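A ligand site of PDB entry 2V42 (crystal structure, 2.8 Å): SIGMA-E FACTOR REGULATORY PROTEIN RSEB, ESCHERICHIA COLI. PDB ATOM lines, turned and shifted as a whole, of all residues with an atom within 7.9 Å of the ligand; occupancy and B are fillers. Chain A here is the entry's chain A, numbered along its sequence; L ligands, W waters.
Water W1 bridges the backbone NH of Gln 282 (2.9 Å) and an oxygen (O2) of the ligand (3.1 Å).
O1 of the ligand lies within salt-bridge range of NE of Arg 154, 2.5 Å away.
An oxygen (O2) of the ligand is in salt-bridge range of the guanidinium group of Arg 257 (2.7 Å).
The backbone NH (N) of Arg 154 is in hydrogen-bond range of an oxygen (O3) of the ligand.
The side-chain carboxylate of Asp 153 sits close to an oxygen (O3) of the ligand, at 3.0 Å.
The guanidinium group of Arg 154 sits at hydrogen-bond distance from the backbone carbonyl oxygen of Gly 130.
The side-chain hydroxyl (OH) of Tyr 133 is in hydrogen-bond range of the backbone carbonyl oxygen (O) of Leu 279.
The guanidinium group (NH1) of Arg 257 is in hydrogen-bond range of the side-chain hydroxyl (OH) of Tyr 133 (2.9 Å).
OD2 of Asp 153 is in salt-bridge range of NH2 of Arg 257 (2.8 Å).
The guanidinium group (NH2) of Arg 154 sits at hydrogen-bond distance from the side-chain amide oxygen (OE1) of Gln 282 (3.0 Å).
Merely in contact with the ligand: Tyr 133 (3.7 Å), Asp 155 (3.4 Å), Pro 280 (3.4 Å) and Pro 281 (3.6 Å).
Hydrophobic or aromatic side chains that line the ligand: Tyr 133, Pro 280 and Pro 281.
Seven residues have an atom within 4 Å of the ligand: Tyr 133, Asp 153, Arg 154, Asp 155, Arg 257, Pro 280 and Pro 281.
The nearest printed residue that does not touch the ligand is Gln 282 (5.6 Å).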
ATOM      1  N   GLY A 130      14.634   5.881   0.766  1.00  0.00           N
ATOM      2  CA  GLY A 130      15.288   4.583   1.039  1.00  0.00           C
ATOM      3  C   GLY A 130      15.418   3.662  -0.169  1.00  0.00           C
ATOM      4  O   GLY A 130      15.600   2.452  -0.051  1.00  0.00           O
ATOM      5  N   THR A 131      15.381   4.276  -1.334  1.00  0.00           N
ATOM      6  CA  THR A 131      15.103   3.614  -2.580  1.00  0.00           C
ATOM      7  C   THR A 131      16.359   3.334  -3.445  1.00  0.00           C
ATOM      8  O   THR A 131      16.341   2.456  -4.312  1.00  0.00           O
ATOM      9  CB  THR A 131      14.065   4.495  -3.326  1.00  0.00           C
ATOM     10  OG1 THR A 131      12.773   3.855  -3.324  1.00  0.00           O
ATOM     11  CG2 THR A 131      14.472   4.793  -4.728  1.00  0.00           C
ATOM     12  N   ARG A 132      17.443   4.079  -3.193  1.00  0.00           N
ATOM     13  CA  ARG A 132      18.640   4.061  -4.039  1.00  0.00           C
ATOM     14  C   ARG A 132      19.903   3.688  -3.269  1.00  0.00           C
ATOM     15  O   ARG A 132      19.875   3.563  -2.043  1.00  0.00           O
ATOM     16  CB  ARG A 132      18.897   5.459  -4.631  1.00  0.00           C
ATOM     17  CG  ARG A 132      17.919   5.964  -5.710  1.00  0.00           C
ATOM     18  CD  ARG A 132      16.909   6.874  -5.071  1.00  0.00           C
ATOM     19  NE  ARG A 132      16.657   8.101  -5.790  1.00  0.00           N
ATOM     20  CZ  ARG A 132      15.611   8.904  -5.561  1.00  0.00           C
ATOM     21  NH1 ARG A 132      14.702   8.601  -4.628  1.00  0.00           N
ATOM     22  NH2 ARG A 132      15.466  10.008  -6.274  1.00  0.00           N
ATOM     23  N   TYR A 133      21.006   3.526  -3.990  1.00  0.00           N
ATOM     24  CA  TYR A 133      22.334   3.467  -3.396  1.00  0.00           C
ATOM     25  C   TYR A 133      22.651   4.861  -2.837  1.00  0.00           C
ATOM     26  O   TYR A 133      21.928   5.834  -3.103  1.00  0.00           O
ATOM     27  CB  TYR A 133      23.352   3.114  -4.466  1.00  0.00           C
ATOM     28  CG  TYR A 133      23.109   1.810  -5.153  1.00  0.00           C
ATOM     29  CD1 TYR A 133      22.497   0.737  -4.497  1.00  0.00           C
ATOM     30  CD2 TYR A 133      23.512   1.611  -6.472  1.00  0.00           C
ATOM     31  CE1 TYR A 133      22.285  -0.464  -5.126  1.00  0.00           C
ATOM     32  CE2 TYR A 133      23.297   0.416  -7.109  1.00  0.00           C
ATOM     33  CZ  TYR A 133      22.681  -0.628  -6.433  1.00  0.00           C
ATOM     34  OH  TYR A 133      22.471  -1.846  -7.061  1.00  0.00           O
ATOM     35  N   SER A 134      23.717   4.970  -2.053  1.00  0.00           N
ATOM     36  CA  SER A 134      24.125   6.272  -1.536  1.00  0.00           C
ATOM     37  C   SER A 134      25.601   6.487  -1.759  1.00  0.00           C
ATOM     38  O   SER A 134      26.338   5.561  -2.116  1.00  0.00           O
ATOM     39  CB  SER A 134      23.809   6.419  -0.056  1.00  0.00           C
ATOM     40  OG  SER A 134      24.649   5.567   0.676  1.00  0.00           O
ATOM     41  N   LEU A 152      27.723   3.217  -2.127  1.00  0.00           N
ATOM     42  CA  LEU A 152      27.354   2.209  -1.149  1.00  0.00           C
ATOM     43  C   LEU A 152      26.014   1.512  -1.407  1.00  0.00           C
ATOM     44  O   LEU A 152      25.025   2.145  -1.797  1.00  0.00           O
ATOM     45  CB  LEU A 152      27.314   2.853   0.244  1.00  0.00           C
ATOM     46  CG  LEU A 152      28.566   3.495   0.844  1.00  0.00           C
ATOM     47  CD1 LEU A 152      28.217   4.105   2.182  1.00  0.00           C
ATOM     48  CD2 LEU A 152      29.649   2.446   1.012  1.00  0.00           C
ATOM     49  N   ASP A 153      25.983   0.205  -1.181  1.00  0.00           N
ATOM     50  CA  ASP A 153      24.762  -0.568  -0.993  1.00  0.00           C
ATOM     51  C   ASP A 153      23.804   0.110  -0.064  1.00  0.00           C
ATOM     52  O   ASP A 153      24.185   0.965   0.726  1.00  0.00           O
ATOM     53  CB  ASP A 153      25.083  -1.913  -0.300  1.00  0.00           C
ATOM     54  CG  ASP A 153      25.011  -3.081  -1.229  1.00  0.00           C
ATOM     55  OD1 ASP A 153      25.482  -4.171  -0.843  1.00  0.00           O
ATOM     56  OD2 ASP A 153      24.474  -2.932  -2.334  1.00  0.00           O
ATOM     57  N   ARG A 154      22.555  -0.348  -0.118  1.00  0.00           N
ATOM     58  CA  ARG A 154      21.571  -0.022   0.910  1.00  0.00           C
ATOM     59  C   ARG A 154      21.919  -0.697   2.240  1.00  0.00           C
ATOM     60  O   ARG A 154      21.475  -0.271   3.300  1.00  0.00           O
ATOM     61  CB  ARG A 154      20.149  -0.299   0.410  1.00  0.00           C
ATOM     62  CG  ARG A 154      19.774   0.598  -0.775  1.00  0.00           C
ATOM     63  CD  ARG A 154      18.291   0.634  -1.095  1.00  0.00           C
ATOM     64  NE  ARG A 154      17.773  -0.686  -1.486  1.00  0.00           N
ATOM     65  CZ  ARG A 154      16.482  -0.983  -1.669  1.00  0.00           C
ATOM     66  NH1 ARG A 154      15.554  -0.057  -1.534  1.00  0.00           N
ATOM     67  NH2 ARG A 154      16.134  -2.217  -2.011  1.00  0.00           N
ATOM     68  N   ASP A 155      22.764  -1.733   2.173  1.00  0.00           N
ATOM     69  CA  ASP A 155      23.296  -2.390   3.352  1.00  0.00           C
ATOM     70  C   ASP A 155      24.673  -1.875   3.788  1.00  0.00           C
ATOM     71  O   ASP A 155      25.326  -2.485   4.633  1.00  0.00           O
ATOM     72  CB  ASP A 155      23.381  -3.897   3.106  1.00  0.00           C
ATOM     73  CG  ASP A 155      22.018  -4.549   2.886  1.00  0.00           C
ATOM     74  OD1 ASP A 155      20.983  -3.989   3.338  1.00  0.00           O
ATOM     75  OD2 ASP A 155      21.992  -5.641   2.266  1.00  0.00           O
ATOM     76  N   GLY A 156      25.124  -0.763   3.202  1.00  0.00           N
ATOM     77  CA  GLY A 156      26.424  -0.194   3.538  1.00  0.00           C
ATOM     78  C   GLY A 156      27.660  -0.828   2.918  1.00  0.00           C
ATOM     79  O   GLY A 156      28.778  -0.365   3.158  1.00  0.00           O
ATOM     80  N   GLU A 157      27.490  -1.874   2.116  1.00  0.00           N
ATOM     81  CA  GLU A 157      28.606  -2.481   1.393  1.00  0.00           C
ATOM     82  C   GLU A 157      29.086  -1.565   0.290  1.00  0.00           C
ATOM     83  O   GLU A 157      28.270  -1.031  -0.449  1.00  0.00           O
ATOM     84  CB  GLU A 157      28.212  -3.814   0.763  1.00  0.00           C
ATOM     85  CG  GLU A 157      27.844  -4.908   1.771  1.00  0.00           C
ATOM     86  CD  GLU A 157      28.924  -5.121   2.822  1.00  0.00           C
ATOM     87  OE1 GLU A 157      29.923  -5.797   2.493  1.00  0.00           O
ATOM     88  OE2 GLU A 157      28.766  -4.593   3.953  1.00  0.00           O
ATOM     89  N   LEU A 159      30.278  -0.505  -3.245  1.00  0.00           N
ATOM     90  CA  LEU A 159      30.255  -0.986  -4.632  1.00  0.00           C
ATOM     91  C   LEU A 159      31.408  -0.445  -5.477  1.00  0.00           C
ATOM     92  O   LEU A 159      31.879  -1.108  -6.405  1.00  0.00           O
ATOM     93  CB  LEU A 159      28.947  -0.568  -5.319  1.00  0.00           C
ATOM     94  CG  LEU A 159      27.599  -1.202  -4.945  1.00  0.00           C
ATOM     95  CD1 LEU A 159      26.453  -0.391  -5.550  1.00  0.00           C
ATOM     96  CD2 LEU A 159      27.494  -2.672  -5.327  1.00  0.00           C
ATOM     97  N   ARG A 257      22.608  -8.123 -11.581  1.00  0.00           N
ATOM     98  CA  ARG A 257      23.336  -6.990 -11.049  1.00  0.00           C
ATOM     99  C   ARG A 257      24.816  -7.291 -11.093  1.00  0.00           C
ATOM    100  O   ARG A 257      25.283  -8.284 -10.540  1.00  0.00           O
ATOM    101  CB  ARG A 257      22.898  -6.640  -9.630  1.00  0.00           C
ATOM    102  CG  ARG A 257      24.004  -6.005  -8.796  1.00  0.00           C
ATOM    103  CD  ARG A 257      23.457  -5.221  -7.662  1.00  0.00           C
ATOM    104  NE  ARG A 257      24.230  -5.381  -6.433  1.00  0.00           N
ATOM    105  CZ  ARG A 257      23.911  -4.819  -5.262  1.00  0.00           C
ATOM    106  NH1 ARG A 257      22.827  -4.041  -5.173  1.00  0.00           N
ATOM    107  NH2 ARG A 257      24.661  -5.020  -4.177  1.00  0.00           N
ATOM    108  N   THR A 262      22.242  -2.614 -13.105  1.00  0.00           N
ATOM    109  CA  THR A 262      21.215  -3.583 -12.839  1.00  0.00           C
ATOM    110  C   THR A 262      20.430  -3.750 -14.120  1.00  0.00           C
ATOM    111  O   THR A 262      20.005  -2.749 -14.706  1.00  0.00           O
ATOM    112  CB  THR A 262      20.276  -3.083 -11.735  1.00  0.00           C
ATOM    113  OG1 THR A 262      21.056  -2.769 -10.580  1.00  0.00           O
ATOM    114  CG2 THR A 262      19.248  -4.142 -11.366  1.00  0.00           C
ATOM    115  N   LEU A 279      20.419   1.202 -10.063  1.00  0.00           N
ATOM    116  CA  LEU A 279      19.331   1.082  -9.110  1.00  0.00           C
ATOM    117  C   LEU A 279      19.423  -0.234  -8.358  1.00  0.00           C
ATOM    118  O   LEU A 279      19.833  -1.235  -8.927  1.00  0.00           O
ATOM    119  CB  LEU A 279      18.005   1.114  -9.836  1.00  0.00           C
ATOM    120  CG  LEU A 279      17.515   2.388 -10.469  1.00  0.00           C
ATOM    121  CD1 LEU A 279      16.167   2.060 -11.139  1.00  0.00           C
ATOM    122  CD2 LEU A 279      17.389   3.495  -9.450  1.00  0.00           C
ATOM    123  N   PRO A 280      19.056  -0.236  -7.072  1.00  0.00           N
ATOM    124  CA  PRO A 280      18.875  -1.514  -6.388  1.00  0.00           C
ATOM    125  C   PRO A 280      17.873  -2.365  -7.151  1.00  0.00           C
ATOM    126  O   PRO A 280      16.836  -1.869  -7.566  1.00  0.00           O
ATOM    127  CB  PRO A 280      18.287  -1.099  -5.036  1.00  0.00           C
ATOM    128  CG  PRO A 280      18.819   0.281  -4.809  1.00  0.00           C
ATOM    129  CD  PRO A 280      18.832   0.911  -6.180  1.00  0.00           C
ATOM    130  N   PRO A 281      18.197  -3.642  -7.375  1.00  0.00           N
ATOM    131  CA  PRO A 281      17.285  -4.618  -7.940  1.00  0.00           C
ATOM    132  C   PRO A 281      15.821  -4.455  -7.520  1.00  0.00           C
ATOM    133  O   PRO A 281      14.948  -4.300  -8.381  1.00  0.00           O
ATOM    134  CB  PRO A 281      17.865  -5.933  -7.416  1.00  0.00           C
ATOM    135  CG  PRO A 281      19.318  -5.697  -7.455  1.00  0.00           C
ATOM    136  CD  PRO A 281      19.531  -4.226  -7.133  1.00  0.00           C
ATOM    137  N   GLN A 282      15.548  -4.460  -6.218  1.00  0.00           N
ATOM    138  CA  GLN A 282      14.188  -4.257  -5.706  1.00  0.00           C
ATOM    139  C   GLN A 282      13.483  -3.055  -6.363  1.00  0.00           C
ATOM    140  O   GLN A 282      12.340  -3.179  -6.831  1.00  0.00           O
ATOM    141  CB  GLN A 282      14.219  -4.102  -4.176  1.00  0.00           C
ATOM    142  CG  GLN A 282      12.829  -4.111  -3.496  1.00  0.00           C
ATOM    143  CD  GLN A 282      12.798  -3.352  -2.167  1.00  0.00           C
ATOM    144  OE1 GLN A 282      13.130  -2.162  -2.099  1.00  0.00           O
ATOM    145  NE2 GLN A 282      12.405  -4.047  -1.109  1.00  0.00           N
ATOM    146  N   THR A 283      14.160  -1.902  -6.413  1.00  0.00           N
ATOM    147  CA  THR A 283      13.599  -0.698  -7.005  1.00  0.00           C
ATOM    148  C   THR A 283      13.315  -0.868  -8.496  1.00  0.00           C
ATOM    149  O   THR A 283      12.276  -0.427  -8.984  1.00  0.00           O
ATOM    150  CB  THR A 283      14.504   0.529  -6.808  1.00  0.00           C
ATOM    151  OG1 THR A 283      14.723   0.720  -5.406  1.00  0.00           O
ATOM    152  CG2 THR A 283      13.844   1.784  -7.345  1.00  0.00           C
HETATM  153  O1  LIG L   1      19.208  -2.597  -2.151  1.00  0.00           O
HETATM  154  S1  LIG L   1      20.519  -3.264  -2.293  1.00  0.00           S
HETATM  155  O2  LIG L   1      20.610  -3.718  -3.689  1.00  0.00           O
HETATM  156  O3  LIG L   1      21.565  -2.277  -1.979  1.00  0.00           O
HETATM  157  C1  LIG L   1      20.676  -4.525  -1.226  1.00  0.00           C
HETATM  158  C2  LIG L   1      21.529  -5.638  -1.822  1.00  0.00           C
HETATM  159  C3  LIG L   1      21.611  -6.852  -0.898  1.00  0.00           C
HETATM  160  N1  LIG L   1      20.916  -8.108  -1.348  1.00  0.00           N
HETATM  161  C4  LIG L   1      20.008  -7.952  -2.509  1.00  0.00           C
HETATM  162  C5  LIG L   1      21.983  -9.058  -1.746  1.00  0.00           C
HETATM  163  C6  LIG L   1      20.181  -8.673  -0.187  1.00  0.00           C
HETATM  164  C7  LIG L   1      18.960  -7.896   0.297  1.00  0.00           C
HETATM  165  O   HOH W   1      17.700  -4.598  -4.345  1.00  0.00           O
